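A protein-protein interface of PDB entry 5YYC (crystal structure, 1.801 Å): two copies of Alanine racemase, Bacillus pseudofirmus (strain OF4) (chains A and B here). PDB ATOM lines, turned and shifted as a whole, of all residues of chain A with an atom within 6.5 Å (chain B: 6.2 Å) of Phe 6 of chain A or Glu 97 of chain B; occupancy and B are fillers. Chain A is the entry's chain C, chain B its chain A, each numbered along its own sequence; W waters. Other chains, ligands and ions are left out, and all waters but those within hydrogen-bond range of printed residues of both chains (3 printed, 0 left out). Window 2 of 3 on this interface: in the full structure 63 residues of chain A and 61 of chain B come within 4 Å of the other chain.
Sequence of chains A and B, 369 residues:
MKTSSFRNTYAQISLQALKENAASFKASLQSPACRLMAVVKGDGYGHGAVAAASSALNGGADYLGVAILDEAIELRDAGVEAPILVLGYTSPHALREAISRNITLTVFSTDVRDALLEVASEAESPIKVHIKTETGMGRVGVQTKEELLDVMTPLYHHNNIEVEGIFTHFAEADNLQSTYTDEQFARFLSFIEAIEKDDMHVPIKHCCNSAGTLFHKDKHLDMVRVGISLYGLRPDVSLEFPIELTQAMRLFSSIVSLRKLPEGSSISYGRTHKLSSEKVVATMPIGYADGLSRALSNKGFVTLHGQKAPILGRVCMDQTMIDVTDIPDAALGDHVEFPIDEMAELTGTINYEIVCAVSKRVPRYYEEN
The side-chain carboxylate (OD2) of Asp 70 of chain B is in salt-bridge range of the side-chain amino group (NZ) of Lys 2 of chain A (2.8 Å).
The side-chain hydroxyl of Ser 5 of chain A sits at hydrogen-bond distance from the side-chain carboxylate of Asp 70 of chain B.
The backbone NH (N) of Phe 6 of chain A is in hydrogen-bond range of the side-chain carboxylate (OD1) of Asp 70 of chain B (3.0 Å).
Of the 15 printed residues of chain B, 6 touch a printed residue of chain A.
Printed residues of chain B that touch a printed residue of chain A: Asp 70, Ile 73, Ser 91, His 93, Ala 94 and Glu 97.
Hydrophobic or aromatic side chains of chain B that line the printed part of chain A: Ile 73, His 93 and Ala 94.
Of the 7 printed residues of chain A, 3 touch a printed residue of chain B.
Hydrophobic or aromatic side chains of chain A within 4 Å of the printed part of chain B: Phe 6.
Among the printed residues, 8 pairs touch across the chains.
A ring nitrogen (ND1) of His 93 of chain B lies within hydrogen-bond range of the side-chain hydroxyl of Ser 91 of chain B, 2.7 Å away.
The side-chain hydroxyl of Ser 100 of chain B sits at hydrogen-bond distance from the backbone carbonyl oxygen of Glu 97 of chain B (2.9 Å).
The backbone NH (N) of Arg 7 of chain A sits at hydrogen-bond distance from the side-chain hydroxyl (OG) of Ser 5 of chain A.
Water W1 bridges the backbone carbonyl oxygen (O) of Ser 5 of chain A (2.7 Å) and a ring nitrogen (NE2) of His 93 of chain B (2.9 Å).
Water W2 lies within hydrogen-bond range of OG of Ser 91 of chain B (2.9 Å) and O of Phe 6 of chain A (2.9 Å).
Water W3 bridges N of Ser 91 of chain B and O of Phe 6 of chain A.
Of the printed residues of chain B, Lys 2 of chain A touches Asp 70 (2.8 Å).
Printed residues of chain B within 4 Å of Ser 5 of chain A: Asp 70.
Printed residues of chain A within 4 Å of Ser 91 of chain B: Phe 6 (3.8 Å).
Printed residues of chain A within 4 Å of His 93 of chain B: Phe 6 (3.2 Å).
Leu 95 of chain B touches none of the printed residues of chain A.
Glu 97 of chain B touches just one residue of chain A: Phe 6 (3.5 Å).
Arg 101 of chain B touches none of the printed residues of chain A.
The nearest printed residue of chain A that does not touch Glu 97 of chain B is Ser 5 of chain A (9.1 Å).
Phe 6 of chain A touches Ile 73 of chain B (CE2 to CD1, 3.5 Å).
OG of Ser 91 of chain B touches O of Phe 6 of chain A (3.8 Å).
CE1 of His 93 of chain B touches O of Phe 6 of chain A, 3.2 Å away.
Ala 94 of chain B touches Phe 6 of chain A.
Phe 6 of chain A touches Glu 97 of chain B.
No position is printed for both chains.
Of the 8 pairs that touch across the chains among the printed residues, none has its exchanged pair printed and touching as well.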
ATOM      1  N   LYS A   2     -11.760 -18.083  21.870  1.00  0.00           N
ATOM      2  CA  LYS A   2     -13.122 -17.739  22.226  1.00  0.00           C
ATOM      3  C   LYS A   2     -13.187 -16.264  22.638  1.00  0.00           C
ATOM      4  O   LYS A   2     -12.428 -15.810  23.496  1.00  0.00           O
ATOM      5  CB  LYS A   2     -13.616 -18.654  23.341  1.00  0.00           C
ATOM      6  CG  LYS A   2     -15.058 -18.406  23.762  1.00  0.00           C
ATOM      7  CD  LYS A   2     -15.455 -19.471  24.781  1.00  0.00           C
ATOM      8  CE  LYS A   2     -16.843 -19.251  25.325  1.00  0.00           C
ATOM      9  NZ  LYS A   2     -17.205 -20.375  26.248  1.00  0.00           N
ATOM     10  N   SER A   4     -16.531 -14.530  22.647  1.00  0.00           N
ATOM     11  CA  SER A   4     -17.888 -14.156  23.032  1.00  0.00           C
ATOM     12  C   SER A   4     -18.480 -15.264  23.892  1.00  0.00           C
ATOM     13  O   SER A   4     -18.020 -16.403  23.849  1.00  0.00           O
ATOM     14  CB  SER A   4     -18.766 -13.893  21.804  1.00  0.00           C
ATOM     15  OG  SER A   4     -19.001 -15.087  21.098  1.00  0.00           O
ATOM     16  N   SER A   5     -19.490 -14.922  24.674  1.00  0.00           N
ATOM     17  CA  SER A   5     -20.082 -15.876  25.606  1.00  0.00           C
ATOM     18  C   SER A   5     -21.422 -15.356  26.103  1.00  0.00           C
ATOM     19  O   SER A   5     -21.652 -14.152  26.127  1.00  0.00           O
ATOM     20  CB  SER A   5     -19.146 -16.118  26.799  1.00  0.00           C
ATOM     21  OG  SER A   5     -19.748 -17.000  27.728  1.00  0.00           O
ATOM     22  N   PHE A   6     -22.301 -16.269  26.502  1.00  0.00           N
ATOM     23  CA  PHE A   6     -23.558 -15.877  27.121  1.00  0.00           C
ATOM     24  C   PHE A   6     -23.427 -15.805  28.643  1.00  0.00           C
ATOM     25  O   PHE A   6     -24.373 -15.423  29.321  1.00  0.00           O
ATOM     26  CB  PHE A   6     -24.675 -16.852  26.727  1.00  0.00           C
ATOM     27  CG  PHE A   6     -25.208 -16.607  25.346  1.00  0.00           C
ATOM     28  CD1 PHE A   6     -26.071 -15.547  25.109  1.00  0.00           C
ATOM     29  CD2 PHE A   6     -24.825 -17.404  24.286  1.00  0.00           C
ATOM     30  CE1 PHE A   6     -26.562 -15.293  23.834  1.00  0.00           C
ATOM     31  CE2 PHE A   6     -25.315 -17.157  22.999  1.00  0.00           C
ATOM     32  CZ  PHE A   6     -26.179 -16.099  22.779  1.00  0.00           C
ATOM     33  N   ARG A   7     -22.251 -16.168  29.157  1.00  0.00           N
ATOM     34  CA  ARG A   7     -21.963 -16.189  30.596  1.00  0.00           C
ATOM     35  C   ARG A   7     -21.001 -15.057  30.962  1.00  0.00           C
ATOM     36  O   ARG A   7     -20.015 -14.838  30.254  1.00  0.00           O
ATOM     37  CB  ARG A   7     -21.356 -17.552  30.999  1.00  0.00           C
ATOM     38  CG  ARG A   7     -20.844 -17.662  32.454  1.00  0.00           C
ATOM     39  CD  ARG A   7     -20.168 -19.019  32.671  1.00  0.00           C
ATOM     40  NE  ARG A   7     -18.905 -19.056  31.924  1.00  0.00           N
ATOM     41  CZ  ARG A   7     -17.892 -19.876  32.191  1.00  0.00           C
ATOM     42  NH1 ARG A   7     -17.982 -20.755  33.182  1.00  0.00           N
ATOM     43  NH2 ARG A   7     -16.776 -19.795  31.473  1.00  0.00           N
ATOM     44  N   ASN A   8     -21.287 -14.339  32.050  1.00  0.00           N
ATOM     45  CA  ASN A   8     -20.411 -13.259  32.496  1.00  0.00           C
ATOM     46  C   ASN A   8     -19.256 -13.765  33.358  1.00  0.00           C
ATOM     47  O   ASN A   8     -19.159 -13.484  34.555  1.00  0.00           O
ATOM     48  CB  ASN A   8     -21.213 -12.181  33.235  1.00  0.00           C
ATOM     49  CG  ASN A   8     -21.861 -11.198  32.279  1.00  0.00           C
ATOM     50  OD1 ASN A   8     -21.264 -10.828  31.277  1.00  0.00           O
ATOM     51  ND2 ASN A   8     -23.076 -10.773  32.583  1.00  0.00           N
ATOM     52  N   TYR A 365     -11.919 -10.769  26.032  1.00  0.00           N
ATOM     53  CA  TYR A 365     -12.514  -9.552  25.512  1.00  0.00           C
ATOM     54  C   TYR A 365     -11.416  -8.541  25.300  1.00  0.00           C
ATOM     55  O   TYR A 365     -10.786  -8.086  26.258  1.00  0.00           O
ATOM     56  CB  TYR A 365     -13.558  -9.004  26.481  1.00  0.00           C
ATOM     57  CG  TYR A 365     -14.782  -9.878  26.630  1.00  0.00           C
ATOM     58  CD1 TYR A 365     -15.164 -10.744  25.620  1.00  0.00           C
ATOM     59  CD2 TYR A 365     -15.564  -9.824  27.778  1.00  0.00           C
ATOM     60  CE1 TYR A 365     -16.297 -11.542  25.747  1.00  0.00           C
ATOM     61  CE2 TYR A 365     -16.703 -10.619  27.911  1.00  0.00           C
ATOM     62  CZ  TYR A 365     -17.058 -11.473  26.890  1.00  0.00           C
ATOM     63  OH  TYR A 365     -18.182 -12.266  27.010  1.00  0.00           O
ATOM     64  N   LEU B  69     -24.741 -22.485  28.680  1.00  0.00           N
ATOM     65  CA  LEU B  69     -25.347 -22.427  27.349  1.00  0.00           C
ATOM     66  C   LEU B  69     -24.311 -22.507  26.215  1.00  0.00           C
ATOM     67  O   LEU B  69     -24.582 -23.123  25.171  1.00  0.00           O
ATOM     68  CB  LEU B  69     -26.184 -21.134  27.214  1.00  0.00           C
ATOM     69  CG  LEU B  69     -26.892 -20.966  25.868  1.00  0.00           C
ATOM     70  CD1 LEU B  69     -27.787 -22.195  25.587  1.00  0.00           C
ATOM     71  CD2 LEU B  69     -27.733 -19.690  25.827  1.00  0.00           C
ATOM     72  N   ASP B  70     -23.135 -21.889  26.402  1.00  0.00           N
ATOM     73  CA  ASP B  70     -22.099 -21.907  25.362  1.00  0.00           C
ATOM     74  C   ASP B  70     -21.825 -23.339  24.934  1.00  0.00           C
ATOM     75  O   ASP B  70     -21.648 -23.628  23.753  1.00  0.00           O
ATOM     76  CB  ASP B  70     -20.757 -21.313  25.828  1.00  0.00           C
ATOM     77  CG  ASP B  70     -20.804 -19.823  26.122  1.00  0.00           C
ATOM     78  OD1 ASP B  70     -21.828 -19.148  25.897  1.00  0.00           O
ATOM     79  OD2 ASP B  70     -19.760 -19.329  26.589  1.00  0.00           O
ATOM     80  N   ILE B  73     -24.671 -24.815  22.854  1.00  0.00           N
ATOM     81  CA  ILE B  73     -24.653 -24.281  21.500  1.00  0.00           C
ATOM     82  C   ILE B  73     -23.548 -24.960  20.685  1.00  0.00           C
ATOM     83  O   ILE B  73     -23.739 -25.284  19.515  1.00  0.00           O
ATOM     84  CB  ILE B  73     -24.455 -22.754  21.513  1.00  0.00           C
ATOM     85  CG1 ILE B  73     -25.679 -22.079  22.148  1.00  0.00           C
ATOM     86  CG2 ILE B  73     -24.239 -22.221  20.102  1.00  0.00           C
ATOM     87  CD1 ILE B  73     -25.523 -20.567  22.310  1.00  0.00           C
ATOM     88  N   SER B  91     -28.785 -16.819  31.980  1.00  0.00           N
ATOM     89  CA  SER B  91     -29.330 -15.499  32.287  1.00  0.00           C
ATOM     90  C   SER B  91     -30.513 -15.140  31.387  1.00  0.00           C
ATOM     91  O   SER B  91     -30.684 -15.729  30.324  1.00  0.00           O
ATOM     92  CB  SER B  91     -28.230 -14.436  32.159  1.00  0.00           C
ATOM     93  OG  SER B  91     -27.657 -14.471  30.877  1.00  0.00           O
ATOM     94  N   HIS B  93     -31.006 -12.772  29.307  1.00  0.00           N
ATOM     95  CA  HIS B  93     -30.713 -12.273  27.955  1.00  0.00           C
ATOM     96  C   HIS B  93     -30.382 -13.418  26.988  1.00  0.00           C
ATOM     97  O   HIS B  93     -30.378 -13.223  25.767  1.00  0.00           O
ATOM     98  CB  HIS B  93     -29.561 -11.247  27.976  1.00  0.00           C
ATOM     99  CG  HIS B  93     -28.190 -11.848  27.851  1.00  0.00           C
ATOM    100  ND1 HIS B  93     -27.718 -12.828  28.700  1.00  0.00           N
ATOM    101  CD2 HIS B  93     -27.179 -11.586  26.985  1.00  0.00           C
ATOM    102  CE1 HIS B  93     -26.482 -13.151  28.356  1.00  0.00           C
ATOM    103  NE2 HIS B  93     -26.129 -12.409  27.320  1.00  0.00           N
ATOM    104  N   ALA B  94     -30.115 -14.600  27.538  1.00  0.00           N
ATOM    105  CA  ALA B  94     -29.678 -15.755  26.751  1.00  0.00           C
ATOM    106  C   ALA B  94     -30.816 -16.725  26.428  1.00  0.00           C
ATOM    107  O   ALA B  94     -30.621 -17.683  25.675  1.00  0.00           O
ATOM    108  CB  ALA B  94     -28.564 -16.503  27.488  1.00  0.00           C
ATOM    109  N   LEU B  95     -31.996 -16.483  26.996  1.00  0.00           N
ATOM    110  CA  LEU B  95     -33.086 -17.460  26.922  1.00  0.00           C
ATOM    111  C   LEU B  95     -33.603 -17.696  25.499  1.00  0.00           C
ATOM    112  O   LEU B  95     -33.860 -18.837  25.112  1.00  0.00           O
ATOM    113  CB  LEU B  95     -34.252 -17.023  27.816  1.00  0.00           C
ATOM    114  CG  LEU B  95     -33.968 -16.904  29.312  1.00  0.00           C
ATOM    115  CD1 LEU B  95     -35.202 -16.379  30.034  1.00  0.00           C
ATOM    116  CD2 LEU B  95     -33.498 -18.245  29.888  1.00  0.00           C
ATOM    117  N   ARG B  96     -33.769 -16.627  24.726  1.00  0.00           N
ATOM    118  CA  ARG B  96     -34.274 -16.772  23.358  1.00  0.00           C
ATOM    119  C   ARG B  96     -33.322 -17.606  22.499  1.00  0.00           C
ATOM    120  O   ARG B  96     -33.765 -18.464  21.724  1.00  0.00           O
ATOM    121  CB  ARG B  96     -34.508 -15.402  22.716  1.00  0.00           C
ATOM    122  CG  ARG B  96     -35.717 -14.665  23.276  1.00  0.00           C
ATOM    123  CD  ARG B  96     -35.915 -13.338  22.558  1.00  0.00           C
ATOM    124  NE  ARG B  96     -37.202 -12.714  22.872  1.00  0.00           N
ATOM    125  CZ  ARG B  96     -37.379 -11.759  23.780  1.00  0.00           C
ATOM    126  NH1 ARG B  96     -36.353 -11.303  24.488  1.00  0.00           N
ATOM    127  NH2 ARG B  96     -38.590 -11.256  23.978  1.00  0.00           N
ATOM    128  N   GLU B  97     -32.018 -17.368  22.646  1.00  0.00           N
ATOM    129  CA  GLU B  97     -31.021 -18.177  21.940  1.00  0.00           C
ATOM    130  C   GLU B  97     -31.142 -19.654  22.331  1.00  0.00           C
ATOM    131  O   GLU B  97     -31.110 -20.541  21.472  1.00  0.00           O
ATOM    132  CB  GLU B  97     -29.604 -17.676  22.232  1.00  0.00           C
ATOM    133  CG  GLU B  97     -28.548 -18.294  21.341  1.00  0.00           C
ATOM    134  CD  GLU B  97     -28.742 -17.917  19.887  1.00  0.00           C
ATOM    135  OE1 GLU B  97     -29.134 -16.763  19.627  1.00  0.00           O
ATOM    136  OE2 GLU B  97     -28.530 -18.779  19.009  1.00  0.00           O
ATOM    137  N   ALA B  98     -31.269 -19.919  23.628  1.00  0.00           N
ATOM    138  CA  ALA B  98     -31.375 -21.290  24.105  1.00  0.00           C
ATOM    139  C   ALA B  98     -32.609 -21.975  23.534  1.00  0.00           C
ATOM    140  O   ALA B  98     -32.543 -23.124  23.081  1.00  0.00           O
ATOM    141  CB  ALA B  98     -31.416 -21.332  25.641  1.00  0.00           C
ATOM    142  N   ILE B  99     -33.740 -21.280  23.557  1.00  0.00           N
ATOM    143  CA  ILE B  99     -34.976 -21.925  23.133  1.00  0.00           C
ATOM    144  C   ILE B  99     -34.958 -22.119  21.618  1.00  0.00           C
ATOM    145  O   ILE B  99     -35.531 -23.080  21.104  1.00  0.00           O
ATOM    146  CB  ILE B  99     -36.249 -21.137  23.564  1.00  0.00           C
ATOM    147  CG1 ILE B  99     -36.348 -19.789  22.862  1.00  0.00           C
ATOM    148  CG2 ILE B  99     -36.306 -20.968  25.079  1.00  0.00           C
ATOM    149  CD1 ILE B  99     -37.478 -19.716  21.872  1.00  0.00           C
ATOM    150  N   SER B 100     -34.261 -21.245  20.906  1.00  0.00           N
ATOM    151  CA  SER B 100     -34.218 -21.364  19.454  1.00  0.00           C
ATOM    152  C   SER B 100     -33.377 -22.575  19.018  1.00  0.00           C
ATOM    153  O   SER B 100     -33.567 -23.097  17.923  1.00  0.00           O
ATOM    154  CB  SER B 100     -33.675 -20.079  18.822  1.00  0.00           C
ATOM    155  OG  SER B 100     -32.259 -20.076  18.804  1.00  0.00           O
ATOM    156  N   ARG B 101     -32.462 -23.023  19.880  1.00  0.00           N
ATOM    157  CA  ARG B 101     -31.628 -24.191  19.581  1.00  0.00           C
ATOM    158  C   ARG B 101     -32.097 -25.440  20.329  1.00  0.00           C
ATOM    159  O   ARG B 101     -31.346 -26.411  20.445  1.00  0.00           O
ATOM    160  CB  ARG B 101     -30.155 -23.937  19.931  1.00  0.00           C
ATOM    161  CG  ARG B 101     -29.484 -22.704  19.309  1.00  0.00           C
ATOM    162  CD  ARG B 101     -29.642 -22.610  17.790  1.00  0.00           C
ATOM    163  NE  ARG B 101     -29.011 -23.715  17.060  1.00  0.00           N
ATOM    164  CZ  ARG B 101     -27.711 -23.806  16.788  1.00  0.00           C
ATOM    165  NH1 ARG B 101     -26.861 -22.866  17.195  1.00  0.00           N
ATOM    166  NH2 ARG B 101     -27.253 -24.850  16.108  1.00  0.00           N
ATOM    167  N   ASN B 102     -33.321 -25.398  20.848  1.00  0.00           N
ATOM    168  CA  ASN B 102     -33.950 -26.543  21.514  1.00  0.00           C
ATOM    169  C   ASN B 102     -33.120 -27.074  22.682  1.00  0.00           C
ATOM    170  O   ASN B 102     -32.882 -28.276  22.814  1.00  0.00           O
ATOM    171  CB  ASN B 102     -34.221 -27.656  20.499  1.00  0.00           C
ATOM    172  CG  ASN B 102     -35.118 -27.190  19.363  1.00  0.00           C
ATOM    173  OD1 ASN B 102     -34.742 -27.252  18.192  1.00  0.00           O
ATOM    174  ND2 ASN B 102     -36.305 -26.702  19.708  1.00  0.00           N
ATOM    175  N   ILE B 103     -32.682 -26.151  23.527  1.00  0.00           N
ATOM    176  CA  ILE B 103     -31.881 -26.487  24.689  1.00  0.00           C
ATOM    177  C   ILE B 103     -32.753 -26.421  25.929  1.00  0.00           C
ATOM    178  O   ILE B 103     -33.502 -25.462  26.126  1.00  0.00           O
ATOM    179  CB  ILE B 103     -30.664 -25.542  24.799  1.00  0.00           C
ATOM    180  CG1 ILE B 103     -29.707 -25.824  23.629  1.00  0.00           C
ATOM    181  CG2 ILE B 103     -29.932 -25.737  26.129  1.00  0.00           C
ATOM    182  CD1 ILE B 103     -28.867 -24.647  23.228  1.00  0.00           C
HETATM  183  O   HOH W   1     -23.256 -12.205  27.065  1.00  0.00           O
HETATM  184  O   HOH W   2     -24.988 -13.754  31.598  1.00  0.00           O
HETATM  185  O   HOH W   3     -26.024 -17.069  31.208  1.00  0.00           O
